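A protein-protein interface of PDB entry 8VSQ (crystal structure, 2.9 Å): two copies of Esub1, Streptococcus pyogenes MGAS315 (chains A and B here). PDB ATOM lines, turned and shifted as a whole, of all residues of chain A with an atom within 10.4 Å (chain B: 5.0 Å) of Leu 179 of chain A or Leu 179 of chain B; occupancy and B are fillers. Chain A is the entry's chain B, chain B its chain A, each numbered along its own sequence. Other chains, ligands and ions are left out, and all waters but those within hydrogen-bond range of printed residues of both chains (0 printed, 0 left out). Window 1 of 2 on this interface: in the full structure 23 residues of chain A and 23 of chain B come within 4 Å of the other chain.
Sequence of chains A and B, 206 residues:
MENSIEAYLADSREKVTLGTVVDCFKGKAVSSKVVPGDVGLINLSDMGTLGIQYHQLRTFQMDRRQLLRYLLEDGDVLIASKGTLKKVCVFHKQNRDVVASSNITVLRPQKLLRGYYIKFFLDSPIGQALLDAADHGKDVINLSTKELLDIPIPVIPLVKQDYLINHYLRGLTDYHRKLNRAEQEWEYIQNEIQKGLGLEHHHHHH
Printed residues of chain B within 4 Å of Tyr 175 of chain A: Ala 182 (3.3 Å) and Glu 183 (3.2 Å). Of the printed residues of chain B, Lys 178 of chain A touches Ala 182 (3.96 Å). Of chain B, only Leu 179 (3.3 Å) comes within 4 Å of Leu 179 of chain A. Of the printed residues of chain B, Trp 186 of chain A touches Tyr 175 (3.8 Å). Of the printed residues of chain A, Lys 178 of chain B touches Ala 182 and Glu 185. Printed residues of chain A within 4 Å of Leu 179 of chain B: Leu 179. Glu 183 of chain B touches just one residue of chain A: Tyr 175. The nearest residue of chain B that does not touch Leu 179 of chain A is Ala 182 of chain B (4.2 Å).
Among the printed residues, pairs that only touch across the chains: Tyr 175 of chain A with Ala 182 of chain B (3.3 Å), Tyr 175 of chain A with Glu 183 of chain B (3.2 Å), Lys 178 of chain A with Ala 182 of chain B (3.96 Å), Leu 179 of chain A with Leu 179 of chain B (3.3 Å), Ala 182 of chain A with Tyr 175 of chain B (3.4 Å), Ala 182 of chain A with Lys 178 of chain B (3.9 Å), Glu 183 of chain A with Tyr 175 of chain B (3.3 Å) and Trp 186 of chain A with Tyr 175 of chain B (3.8 Å).
OD2 of Asp 174 of chain A lies within salt-bridge range of NZ of Lys 178 of chain A.
Tyr 175 of chain A touches Ala 182 of chain B, and with the chains exchanged Ala 182 of chain A touches Tyr 175 of chain B. Tyr 175 of chain A touches Glu 183 of chain B, and with the chains exchanged Glu 183 of chain A touches Tyr 175 of chain B. Lys 178 of chain A touches Ala 182 of chain B, and with the chains exchanged Ala 182 of chain A touches Lys 178 of chain B. Leu 179 of chain A touches its own counterpart, Leu 179 of chain B. 10 positions are printed for both chains. Of the 9 pairs that touch across the chains among the printed residues, 7 have their exchanged pair printed and touching as well.
Of the 10 printed residues of chain B, 5 touch a printed residue of chain A. Printed residues of chain B that touch a printed residue of chain A: Tyr 175, Lys 178, Leu 179, Ala 182 and Glu 183. Hydrophobic or aromatic side chains of chain B within 4 Å of the printed part of chain A: Tyr 175, Leu 179 and Ala 182. Among the printed residues, Asp or Glu carboxylates within 4 Å of a Lys or Arg side-chain nitrogen of the other chain: Glu 185 of chain A with Lys 178 of chain B (2.6 Å).
The side-chain amino group (NZ) of Lys 178 of chain B is in salt-bridge range of the side-chain carboxylate (OE1) of Glu 185 of chain A (2.6 Å).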
ATOM      1  N   THR A  49     -15.944 -26.631   9.097  1.00  0.00           N
ATOM      2  CA  THR A  49     -14.865 -27.198   9.945  1.00  0.00           C
ATOM      3  C   THR A  49     -15.255 -27.028  11.410  1.00  0.00           C
ATOM      4  O   THR A  49     -15.418 -28.074  12.106  1.00  0.00           O
ATOM      5  CB  THR A  49     -13.515 -26.510   9.716  1.00  0.00           C
ATOM      6  OG1 THR A  49     -13.320 -26.287   8.318  1.00  0.00           O
ATOM      7  CG2 THR A  49     -12.373 -27.329  10.277  1.00  0.00           C
ATOM      8  N   LEU A  50     -15.459 -25.771  11.828  1.00  0.00           N
ATOM      9  CA  LEU A  50     -15.947 -25.430  13.196  1.00  0.00           C
ATOM     10  C   LEU A  50     -17.494 -25.465  13.275  1.00  0.00           C
ATOM     11  O   LEU A  50     -18.071 -24.838  14.209  1.00  0.00           O
ATOM     12  CB  LEU A  50     -15.404 -24.054  13.572  1.00  0.00           C
ATOM     13  CG  LEU A  50     -15.529 -22.996  12.475  1.00  0.00           C
ATOM     14  CD1 LEU A  50     -16.997 -22.644  12.185  1.00  0.00           C
ATOM     15  CD2 LEU A  50     -14.699 -21.764  12.852  1.00  0.00           C
ATOM     16  N   GLY A  51     -18.159 -26.126  12.318  1.00  0.00           N
ATOM     17  CA  GLY A  51     -19.609 -26.405  12.363  1.00  0.00           C
ATOM     18  C   GLY A  51     -20.391 -25.922  11.142  1.00  0.00           C
ATOM     19  O   GLY A  51     -19.840 -25.201  10.274  1.00  0.00           O
ATOM     20  N   GLY A 171     -14.228 -24.384  24.619  1.00  0.00           N
ATOM     21  CA  GLY A 171     -13.129 -24.170  23.650  1.00  0.00           C
ATOM     22  C   GLY A 171     -13.541 -23.622  22.268  1.00  0.00           C
ATOM     23  O   GLY A 171     -12.763 -22.850  21.674  1.00  0.00           O
ATOM     24  N   LEU A 172     -14.676 -24.052  21.731  1.00  0.00           N
ATOM     25  CA  LEU A 172     -15.167 -23.635  20.408  1.00  0.00           C
ATOM     26  C   LEU A 172     -15.696 -22.207  20.465  1.00  0.00           C
ATOM     27  O   LEU A 172     -15.510 -21.494  19.485  1.00  0.00           O
ATOM     28  CB  LEU A 172     -16.291 -24.569  19.982  1.00  0.00           C
ATOM     29  CG  LEU A 172     -16.878 -24.266  18.613  1.00  0.00           C
ATOM     30  CD1 LEU A 172     -15.804 -24.502  17.565  1.00  0.00           C
ATOM     31  CD2 LEU A 172     -18.101 -25.134  18.391  1.00  0.00           C
ATOM     32  N   THR A 173     -16.407 -21.846  21.523  1.00  0.00           N
ATOM     33  CA  THR A 173     -16.964 -20.483  21.713  1.00  0.00           C
ATOM     34  C   THR A 173     -15.810 -19.518  21.984  1.00  0.00           C
ATOM     35  O   THR A 173     -15.916 -18.308  21.693  1.00  0.00           O
ATOM     36  CB  THR A 173     -17.954 -20.438  22.881  1.00  0.00           C
ATOM     37  OG1 THR A 173     -19.077 -21.240  22.535  1.00  0.00           O
ATOM     38  CG2 THR A 173     -18.465 -19.048  23.176  1.00  0.00           C
ATOM     39  N   ASP A 174     -14.777 -20.059  22.606  1.00  0.00           N
ATOM     40  CA  ASP A 174     -13.513 -19.350  22.841  1.00  0.00           C
ATOM     41  C   ASP A 174     -12.886 -19.051  21.485  1.00  0.00           C
ATOM     42  O   ASP A 174     -12.593 -17.900  21.220  1.00  0.00           O
ATOM     43  CB  ASP A 174     -12.597 -20.209  23.695  1.00  0.00           C
ATOM     44  CG  ASP A 174     -11.710 -19.320  24.504  1.00  0.00           C
ATOM     45  OD1 ASP A 174     -12.263 -18.276  24.987  1.00  0.00           O
ATOM     46  OD2 ASP A 174     -10.491 -19.639  24.580  1.00  0.00           O
ATOM     47  N   TYR A 175     -12.721 -20.082  20.667  1.00  0.00           N
ATOM     48  CA  TYR A 175     -12.158 -20.019  19.299  1.00  0.00           C
ATOM     49  C   TYR A 175     -12.885 -18.962  18.493  1.00  0.00           C
ATOM     50  O   TYR A 175     -12.255 -18.170  17.860  1.00  0.00           O
ATOM     51  CB  TYR A 175     -12.354 -21.344  18.589  1.00  0.00           C
ATOM     52  CG  TYR A 175     -11.585 -21.511  17.319  1.00  0.00           C
ATOM     53  CD1 TYR A 175     -10.281 -21.086  17.213  1.00  0.00           C
ATOM     54  CD2 TYR A 175     -12.151 -22.187  16.254  1.00  0.00           C
ATOM     55  CE1 TYR A 175      -9.572 -21.291  16.043  1.00  0.00           C
ATOM     56  CE2 TYR A 175     -11.462 -22.417  15.086  1.00  0.00           C
ATOM     57  CZ  TYR A 175     -10.167 -21.966  14.987  1.00  0.00           C
ATOM     58  OH  TYR A 175      -9.470 -22.209  13.846  1.00  0.00           O
ATOM     59  N   HIS A 176     -14.203 -18.937  18.558  1.00  0.00           N
ATOM     60  CA  HIS A 176     -15.023 -17.954  17.796  1.00  0.00           C
ATOM     61  C   HIS A 176     -14.832 -16.558  18.380  1.00  0.00           C
ATOM     62  O   HIS A 176     -14.930 -15.638  17.652  1.00  0.00           O
ATOM     63  CB  HIS A 176     -16.527 -18.327  17.734  1.00  0.00           C
ATOM     64  CG  HIS A 176     -16.895 -19.369  16.716  1.00  0.00           C
ATOM     65  ND1 HIS A 176     -18.180 -19.530  16.264  1.00  0.00           N
ATOM     66  CD2 HIS A 176     -16.156 -20.322  16.094  1.00  0.00           C
ATOM     67  CE1 HIS A 176     -18.219 -20.545  15.414  1.00  0.00           C
ATOM     68  NE2 HIS A 176     -16.985 -21.044  15.284  1.00  0.00           N
ATOM     69  N   ARG A 177     -14.650 -16.428  19.680  1.00  0.00           N
ATOM     70  CA  ARG A 177     -14.397 -15.132  20.342  1.00  0.00           C
ATOM     71  C   ARG A 177     -13.063 -14.572  19.803  1.00  0.00           C
ATOM     72  O   ARG A 177     -13.005 -13.364  19.477  1.00  0.00           O
ATOM     73  CB  ARG A 177     -14.392 -15.341  21.861  1.00  0.00           C
ATOM     74  CG  ARG A 177     -14.197 -14.053  22.636  1.00  0.00           C
ATOM     75  CD  ARG A 177     -14.526 -14.135  24.101  1.00  0.00           C
ATOM     76  NE  ARG A 177     -14.203 -12.856  24.743  1.00  0.00           N
ATOM     77  CZ  ARG A 177     -14.350 -12.586  26.061  1.00  0.00           C
ATOM     78  NH1 ARG A 177     -14.849 -13.491  26.902  1.00  0.00           N
ATOM     79  NH2 ARG A 177     -13.987 -11.402  26.545  1.00  0.00           N
ATOM     80  N   LYS A 178     -12.046 -15.439  19.674  1.00  0.00           N
ATOM     81  CA  LYS A 178     -10.657 -15.094  19.234  1.00  0.00           C
ATOM     82  C   LYS A 178     -10.657 -14.725  17.743  1.00  0.00           C
ATOM     83  O   LYS A 178      -9.972 -13.747  17.386  1.00  0.00           O
ATOM     84  CB  LYS A 178      -9.678 -16.258  19.441  1.00  0.00           C
ATOM     85  CG  LYS A 178      -9.409 -16.601  20.890  1.00  0.00           C
ATOM     86  CD  LYS A 178      -8.155 -17.378  21.156  1.00  0.00           C
ATOM     87  CE  LYS A 178      -8.468 -18.557  22.042  1.00  0.00           C
ATOM     88  NZ  LYS A 178      -7.217 -19.234  22.421  1.00  0.00           N
ATOM     89  N   LEU A 179     -11.337 -15.528  16.915  1.00  0.00           N
ATOM     90  CA  LEU A 179     -11.374 -15.365  15.455  1.00  0.00           C
ATOM     91  C   LEU A 179     -12.100 -14.071  15.170  1.00  0.00           C
ATOM     92  O   LEU A 179     -11.584 -13.330  14.370  1.00  0.00           O
ATOM     93  CB  LEU A 179     -12.106 -16.519  14.775  1.00  0.00           C
ATOM     94  CG  LEU A 179     -11.407 -17.886  14.816  1.00  0.00           C
ATOM     95  CD1 LEU A 179     -12.179 -18.941  14.023  1.00  0.00           C
ATOM     96  CD2 LEU A 179      -9.975 -17.828  14.328  1.00  0.00           C
ATOM     97  N   ASN A 180     -13.241 -13.809  15.795  1.00  0.00           N
ATOM     98  CA  ASN A 180     -14.051 -12.623  15.433  1.00  0.00           C
ATOM     99  C   ASN A 180     -13.354 -11.369  15.882  1.00  0.00           C
ATOM    100  O   ASN A 180     -13.527 -10.367  15.237  1.00  0.00           O
ATOM    101  CB  ASN A 180     -15.424 -12.572  16.058  1.00  0.00           C
ATOM    102  CG  ASN A 180     -16.343 -13.526  15.348  1.00  0.00           C
ATOM    103  OD1 ASN A 180     -15.895 -14.374  14.566  1.00  0.00           O
ATOM    104  ND2 ASN A 180     -17.624 -13.375  15.607  1.00  0.00           N
ATOM    105  N   ARG A 181     -12.598 -11.432  16.952  1.00  0.00           N
ATOM    106  CA  ARG A 181     -11.787 -10.271  17.383  1.00  0.00           C
ATOM    107  C   ARG A 181     -10.740  -9.962  16.301  1.00  0.00           C
ATOM    108  O   ARG A 181     -10.659  -8.810  15.820  1.00  0.00           O
ATOM    109  CB  ARG A 181     -11.115 -10.598  18.711  1.00  0.00           C
ATOM    110  CG  ARG A 181     -10.588  -9.363  19.407  1.00  0.00           C
ATOM    111  CD  ARG A 181     -10.285  -9.675  20.847  1.00  0.00           C
ATOM    112  NE  ARG A 181      -9.307 -10.758  20.954  1.00  0.00           N
ATOM    113  CZ  ARG A 181      -9.434 -11.845  21.729  1.00  0.00           C
ATOM    114  NH1 ARG A 181     -10.524 -12.034  22.477  1.00  0.00           N
ATOM    115  NH2 ARG A 181      -8.442 -12.728  21.758  1.00  0.00           N
ATOM    116  N   ALA A 182      -9.980 -10.983  15.920  1.00  0.00           N
ATOM    117  CA  ALA A 182      -8.838 -10.870  15.000  1.00  0.00           C
ATOM    118  C   ALA A 182      -9.331 -10.240  13.700  1.00  0.00           C
ATOM    119  O   ALA A 182      -8.632  -9.365  13.168  1.00  0.00           O
ATOM    120  CB  ALA A 182      -8.210 -12.226  14.792  1.00  0.00           C
ATOM    121  N   GLU A 183     -10.518 -10.641  13.269  1.00  0.00           N
ATOM    122  CA  GLU A 183     -11.177 -10.119  12.059  1.00  0.00           C
ATOM    123  C   GLU A 183     -11.592  -8.674  12.314  1.00  0.00           C
ATOM    124  O   GLU A 183     -11.239  -7.843  11.513  1.00  0.00           O
ATOM    125  CB  GLU A 183     -12.379 -10.975  11.655  1.00  0.00           C
ATOM    126  CG  GLU A 183     -12.704 -10.887  10.169  1.00  0.00           C
ATOM    127  CD  GLU A 183     -13.960 -11.625   9.739  1.00  0.00           C
ATOM    128  OE1 GLU A 183     -14.980 -11.506  10.462  1.00  0.00           O
ATOM    129  OE2 GLU A 183     -13.913 -12.307   8.685  1.00  0.00           O
ATOM    130  N   GLN A 184     -12.296  -8.353  13.386  1.00  0.00           N
ATOM    131  CA  GLN A 184     -12.687  -6.939  13.576  1.00  0.00           C
ATOM    132  C   GLN A 184     -11.410  -6.079  13.544  1.00  0.00           C
ATOM    133  O   GLN A 184     -11.474  -4.949  13.064  1.00  0.00           O
ATOM    134  CB  GLN A 184     -13.446  -6.722  14.876  1.00  0.00           C
ATOM    135  CG  GLN A 184     -14.922  -7.111  14.883  1.00  0.00           C
ATOM    136  CD  GLN A 184     -15.390  -7.085  16.337  1.00  0.00           C
ATOM    137  OE1 GLN A 184     -15.278  -6.048  17.016  1.00  0.00           O
ATOM    138  NE2 GLN A 184     -15.846  -8.228  16.875  1.00  0.00           N
ATOM    139  N   GLU A 185     -10.288  -6.592  14.041  1.00  0.00           N
ATOM    140  CA  GLU A 185      -9.034  -5.807  14.174  1.00  0.00           C
ATOM    141  C   GLU A 185      -8.454  -5.641  12.763  1.00  0.00           C
ATOM    142  O   GLU A 185      -7.958  -4.546  12.433  1.00  0.00           O
ATOM    143  CB  GLU A 185      -8.077  -6.463  15.185  1.00  0.00           C
ATOM    144  CG  GLU A 185      -8.335  -6.055  16.657  1.00  0.00           C
ATOM    145  CD  GLU A 185      -8.010  -7.011  17.829  1.00  0.00           C
ATOM    146  OE1 GLU A 185      -7.359  -8.080  17.638  1.00  0.00           O
ATOM    147  OE2 GLU A 185      -8.427  -6.693  18.970  1.00  0.00           O
ATOM    148  N   TRP A 186      -8.559  -6.681  11.947  1.00  0.00           N
ATOM    149  CA  TRP A 186      -8.061  -6.725  10.551  1.00  0.00           C
ATOM    150  C   TRP A 186      -8.913  -5.819   9.674  1.00  0.00           C
ATOM    151  O   TRP A 186      -8.372  -5.226   8.758  1.00  0.00           O
ATOM    152  CB  TRP A 186      -8.076  -8.161  10.024  1.00  0.00           C
ATOM    153  CG  TRP A 186      -7.802  -8.312   8.562  1.00  0.00           C
ATOM    154  CD1 TRP A 186      -8.518  -9.037   7.650  1.00  0.00           C
ATOM    155  CD2 TRP A 186      -6.692  -7.749   7.845  1.00  0.00           C
ATOM    156  NE1 TRP A 186      -7.923  -8.978   6.421  1.00  0.00           N
ATOM    157  CE2 TRP A 186      -6.805  -8.194   6.513  1.00  0.00           C
ATOM    158  CE3 TRP A 186      -5.598  -6.952   8.211  1.00  0.00           C
ATOM    159  CZ2 TRP A 186      -5.875  -7.826   5.546  1.00  0.00           C
ATOM    160  CZ3 TRP A 186      -4.674  -6.608   7.260  1.00  0.00           C
ATOM    161  CH2 TRP A 186      -4.820  -7.036   5.943  1.00  0.00           C
ATOM    162  N   GLU A 187     -10.207  -5.735   9.934  1.00  0.00           N
ATOM    163  CA  GLU A 187     -11.125  -4.866   9.152  1.00  0.00           C
ATOM    164  C   GLU A 187     -10.854  -3.415   9.513  1.00  0.00           C
ATOM    165  O   GLU A 187     -11.193  -2.538   8.713  1.00  0.00           O
ATOM    166  CB  GLU A 187     -12.598  -5.142   9.442  1.00  0.00           C
ATOM    167  CG  GLU A 187     -13.082  -6.422   8.808  1.00  0.00           C
ATOM    168  CD  GLU A 187     -14.524  -6.758   9.137  1.00  0.00           C
ATOM    169  OE1 GLU A 187     -15.180  -5.933   9.860  1.00  0.00           O
ATOM    170  OE2 GLU A 187     -14.991  -7.845   8.657  1.00  0.00           O
ATOM    171  N   LEU B  50      -8.629 -13.655   2.759  1.00  0.00           N
ATOM    172  CA  LEU B  50      -7.283 -13.160   3.166  1.00  0.00           C
ATOM    173  C   LEU B  50      -6.194 -13.578   2.144  1.00  0.00           C
ATOM    174  O   LEU B  50      -4.981 -13.608   2.518  1.00  0.00           O
ATOM    175  CB  LEU B  50      -6.982 -13.708   4.559  1.00  0.00           C
ATOM    176  CG  LEU B  50      -7.299 -15.192   4.744  1.00  0.00           C
ATOM    177  CD1 LEU B  50      -6.395 -16.090   3.883  1.00  0.00           C
ATOM    178  CD2 LEU B  50      -7.226 -15.555   6.227  1.00  0.00           C
ATOM    179  N   TYR B 175      -2.866 -10.934  11.510  1.00  0.00           N
ATOM    180  CA  TYR B 175      -4.136 -11.688  11.423  1.00  0.00           C
ATOM    181  C   TYR B 175      -3.834 -13.172  11.334  1.00  0.00           C
ATOM    182  O   TYR B 175      -4.441 -13.942  12.025  1.00  0.00           O
ATOM    183  CB  TYR B 175      -4.893 -11.289  10.168  1.00  0.00           C
ATOM    184  CG  TYR B 175      -6.302 -11.789  10.083  1.00  0.00           C
ATOM    185  CD1 TYR B 175      -7.139 -11.763  11.182  1.00  0.00           C
ATOM    186  CD2 TYR B 175      -6.812 -12.226   8.873  1.00  0.00           C
ATOM    187  CE1 TYR B 175      -8.455 -12.178  11.078  1.00  0.00           C
ATOM    188  CE2 TYR B 175      -8.120 -12.629   8.742  1.00  0.00           C
ATOM    189  CZ  TYR B 175      -8.938 -12.603   9.850  1.00  0.00           C
ATOM    190  OH  TYR B 175     -10.231 -12.986   9.693  1.00  0.00           O
ATOM    191  N   HIS B 176      -2.882 -13.554  10.503  1.00  0.00           N
ATOM    192  CA  HIS B 176      -2.527 -14.987  10.310  1.00  0.00           C
ATOM    193  C   HIS B 176      -1.828 -15.517  11.552  1.00  0.00           C
ATOM    194  O   HIS B 176      -1.960 -16.669  11.810  1.00  0.00           O
ATOM    195  CB  HIS B 176      -1.665 -15.239   9.051  1.00  0.00           C
ATOM    196  CG  HIS B 176      -2.425 -15.334   7.759  1.00  0.00           C
ATOM    197  ND1 HIS B 176      -1.950 -16.039   6.680  1.00  0.00           N
ATOM    198  CD2 HIS B 176      -3.623 -14.828   7.379  1.00  0.00           C
ATOM    199  CE1 HIS B 176      -2.805 -15.929   5.679  1.00  0.00           C
ATOM    200  NE2 HIS B 176      -3.842 -15.199   6.086  1.00  0.00           N
ATOM    201  N   ARG B 177      -1.050 -14.704  12.228  1.00  0.00           N
ATOM    202  CA  ARG B 177      -0.374 -15.085  13.483  1.00  0.00           C
ATOM    203  C   ARG B 177      -1.456 -15.411  14.539  1.00  0.00           C
ATOM    204  O   ARG B 177      -1.321 -16.441  15.242  1.00  0.00           O
ATOM    205  CB  ARG B 177       0.560 -13.944  13.905  1.00  0.00           C
ATOM    206  CG  ARG B 177       1.350 -14.258  15.153  1.00  0.00           C
ATOM    207  CD  ARG B 177       2.471 -13.301  15.444  1.00  0.00           C
ATOM    208  NE  ARG B 177       3.012 -13.669  16.764  1.00  0.00           N
ATOM    209  CZ  ARG B 177       4.112 -13.149  17.343  1.00  0.00           C
ATOM    210  NH1 ARG B 177       4.842 -12.226  16.720  1.00  0.00           N
ATOM    211  NH2 ARG B 177       4.472 -13.561  18.555  1.00  0.00           N
ATOM    212  N   LYS B 178      -2.511 -14.584  14.607  1.00  0.00           N
ATOM    213  CA  LYS B 178      -3.634 -14.670  15.590  1.00  0.00           C
ATOM    214  C   LYS B 178      -4.503 -15.893  15.281  1.00  0.00           C
ATOM    215  O   LYS B 178      -4.894 -16.595  16.243  1.00  0.00           O
ATOM    216  CB  LYS B 178      -4.541 -13.432  15.564  1.00  0.00           C
ATOM    217  CG  LYS B 178      -3.888 -12.151  16.039  1.00  0.00           C
ATOM    218  CD  LYS B 178      -4.844 -11.072  16.424  1.00  0.00           C
ATOM    219  CE  LYS B 178      -4.396  -9.766  15.825  1.00  0.00           C
ATOM    220  NZ  LYS B 178      -5.144  -8.658  16.447  1.00  0.00           N
ATOM    221  N   LEU B 179      -4.844 -16.090  14.007  1.00  0.00           N
ATOM    222  CA  LEU B 179      -5.736 -17.173  13.563  1.00  0.00           C
ATOM    223  C   LEU B 179      -5.023 -18.480  13.825  1.00  0.00           C
ATOM    224  O   LEU B 179      -5.664 -19.343  14.350  1.00  0.00           O
ATOM    225  CB  LEU B 179      -6.060 -17.064  12.075  1.00  0.00           C
ATOM    226  CG  LEU B 179      -6.923 -15.876  11.650  1.00  0.00           C
ATOM    227  CD1 LEU B 179      -7.244 -15.942  10.154  1.00  0.00           C
ATOM    228  CD2 LEU B 179      -8.199 -15.772  12.462  1.00  0.00           C
ATOM    229  N   ASN B 180      -3.753 -18.609  13.468  1.00  0.00           N
ATOM    230  CA  ASN B 180      -3.068 -19.916  13.561  1.00  0.00           C
ATOM    231  C   ASN B 180      -2.845 -20.269  15.004  1.00  0.00           C
ATOM    232  O   ASN B 180      -2.845 -21.446  15.290  1.00  0.00           O
ATOM    233  CB  ASN B 180      -1.713 -19.969  12.896  1.00  0.00           C
ATOM    234  CG  ASN B 180      -1.878 -20.096  11.411  1.00  0.00           C
ATOM    235  OD1 ASN B 180      -2.975 -19.901  10.870  1.00  0.00           O
ATOM    236  ND2 ASN B 180      -0.795 -20.454  10.759  1.00  0.00           N
ATOM    237  N   ARG B 181      -2.659 -19.290  15.864  1.00  0.00           N
ATOM    238  CA  ARG B 181      -2.552 -19.560  17.315  1.00  0.00           C
ATOM    239  C   ARG B 181      -3.884 -20.139  17.822  1.00  0.00           C
ATOM    240  O   ARG B 181      -3.902 -21.220  18.443  1.00  0.00           O
ATOM    241  CB  ARG B 181      -2.236 -18.255  18.031  1.00  0.00           C
ATOM    242  CG  ARG B 181      -1.768 -18.470  19.453  1.00  0.00           C
ATOM    243  CD  ARG B 181      -1.114 -17.217  19.964  1.00  0.00           C
ATOM    244  NE  ARG B 181      -2.047 -16.096  19.933  1.00  0.00           N
ATOM    245  CZ  ARG B 181      -1.777 -14.890  19.420  1.00  0.00           C
ATOM    246  NH1 ARG B 181      -0.600 -14.621  18.848  1.00  0.00           N
ATOM    247  NH2 ARG B 181      -2.710 -13.949  19.501  1.00  0.00           N
ATOM    248  N   ALA B 182      -4.976 -19.443  17.529  1.00  0.00           N
ATOM    249  CA  ALA B 182      -6.322 -19.767  18.022  1.00  0.00           C
ATOM    250  C   ALA B 182      -6.657 -21.198  17.601  1.00  0.00           C
ATOM    251  O   ALA B 182      -7.217 -21.931  18.421  1.00  0.00           O
ATOM    252  CB  ALA B 182      -7.303 -18.754  17.493  1.00  0.00           C
ATOM    253  N   GLU B 183      -6.265 -21.572  16.391  1.00  0.00           N
ATOM    254  CA  GLU B 183      -6.461 -22.922  15.845  1.00  0.00           C
ATOM    255  C   GLU B 183      -5.561 -23.894  16.600  1.00  0.00           C
ATOM    256  O   GLU B 183      -6.075 -24.890  17.073  1.00  0.00           O
ATOM    257  CB  GLU B 183      -6.205 -22.963  14.337  1.00  0.00           C
ATOM    258  CG  GLU B 183      -6.940 -24.110  13.640  1.00  0.00           C
ATOM    259  CD  GLU B 183      -6.588 -24.310  12.180  1.00  0.00           C
ATOM    260  OE1 GLU B 183      -5.384 -24.230  11.858  1.00  0.00           O
ATOM    261  OE2 GLU B 183      -7.514 -24.565  11.372  1.00  0.00           O
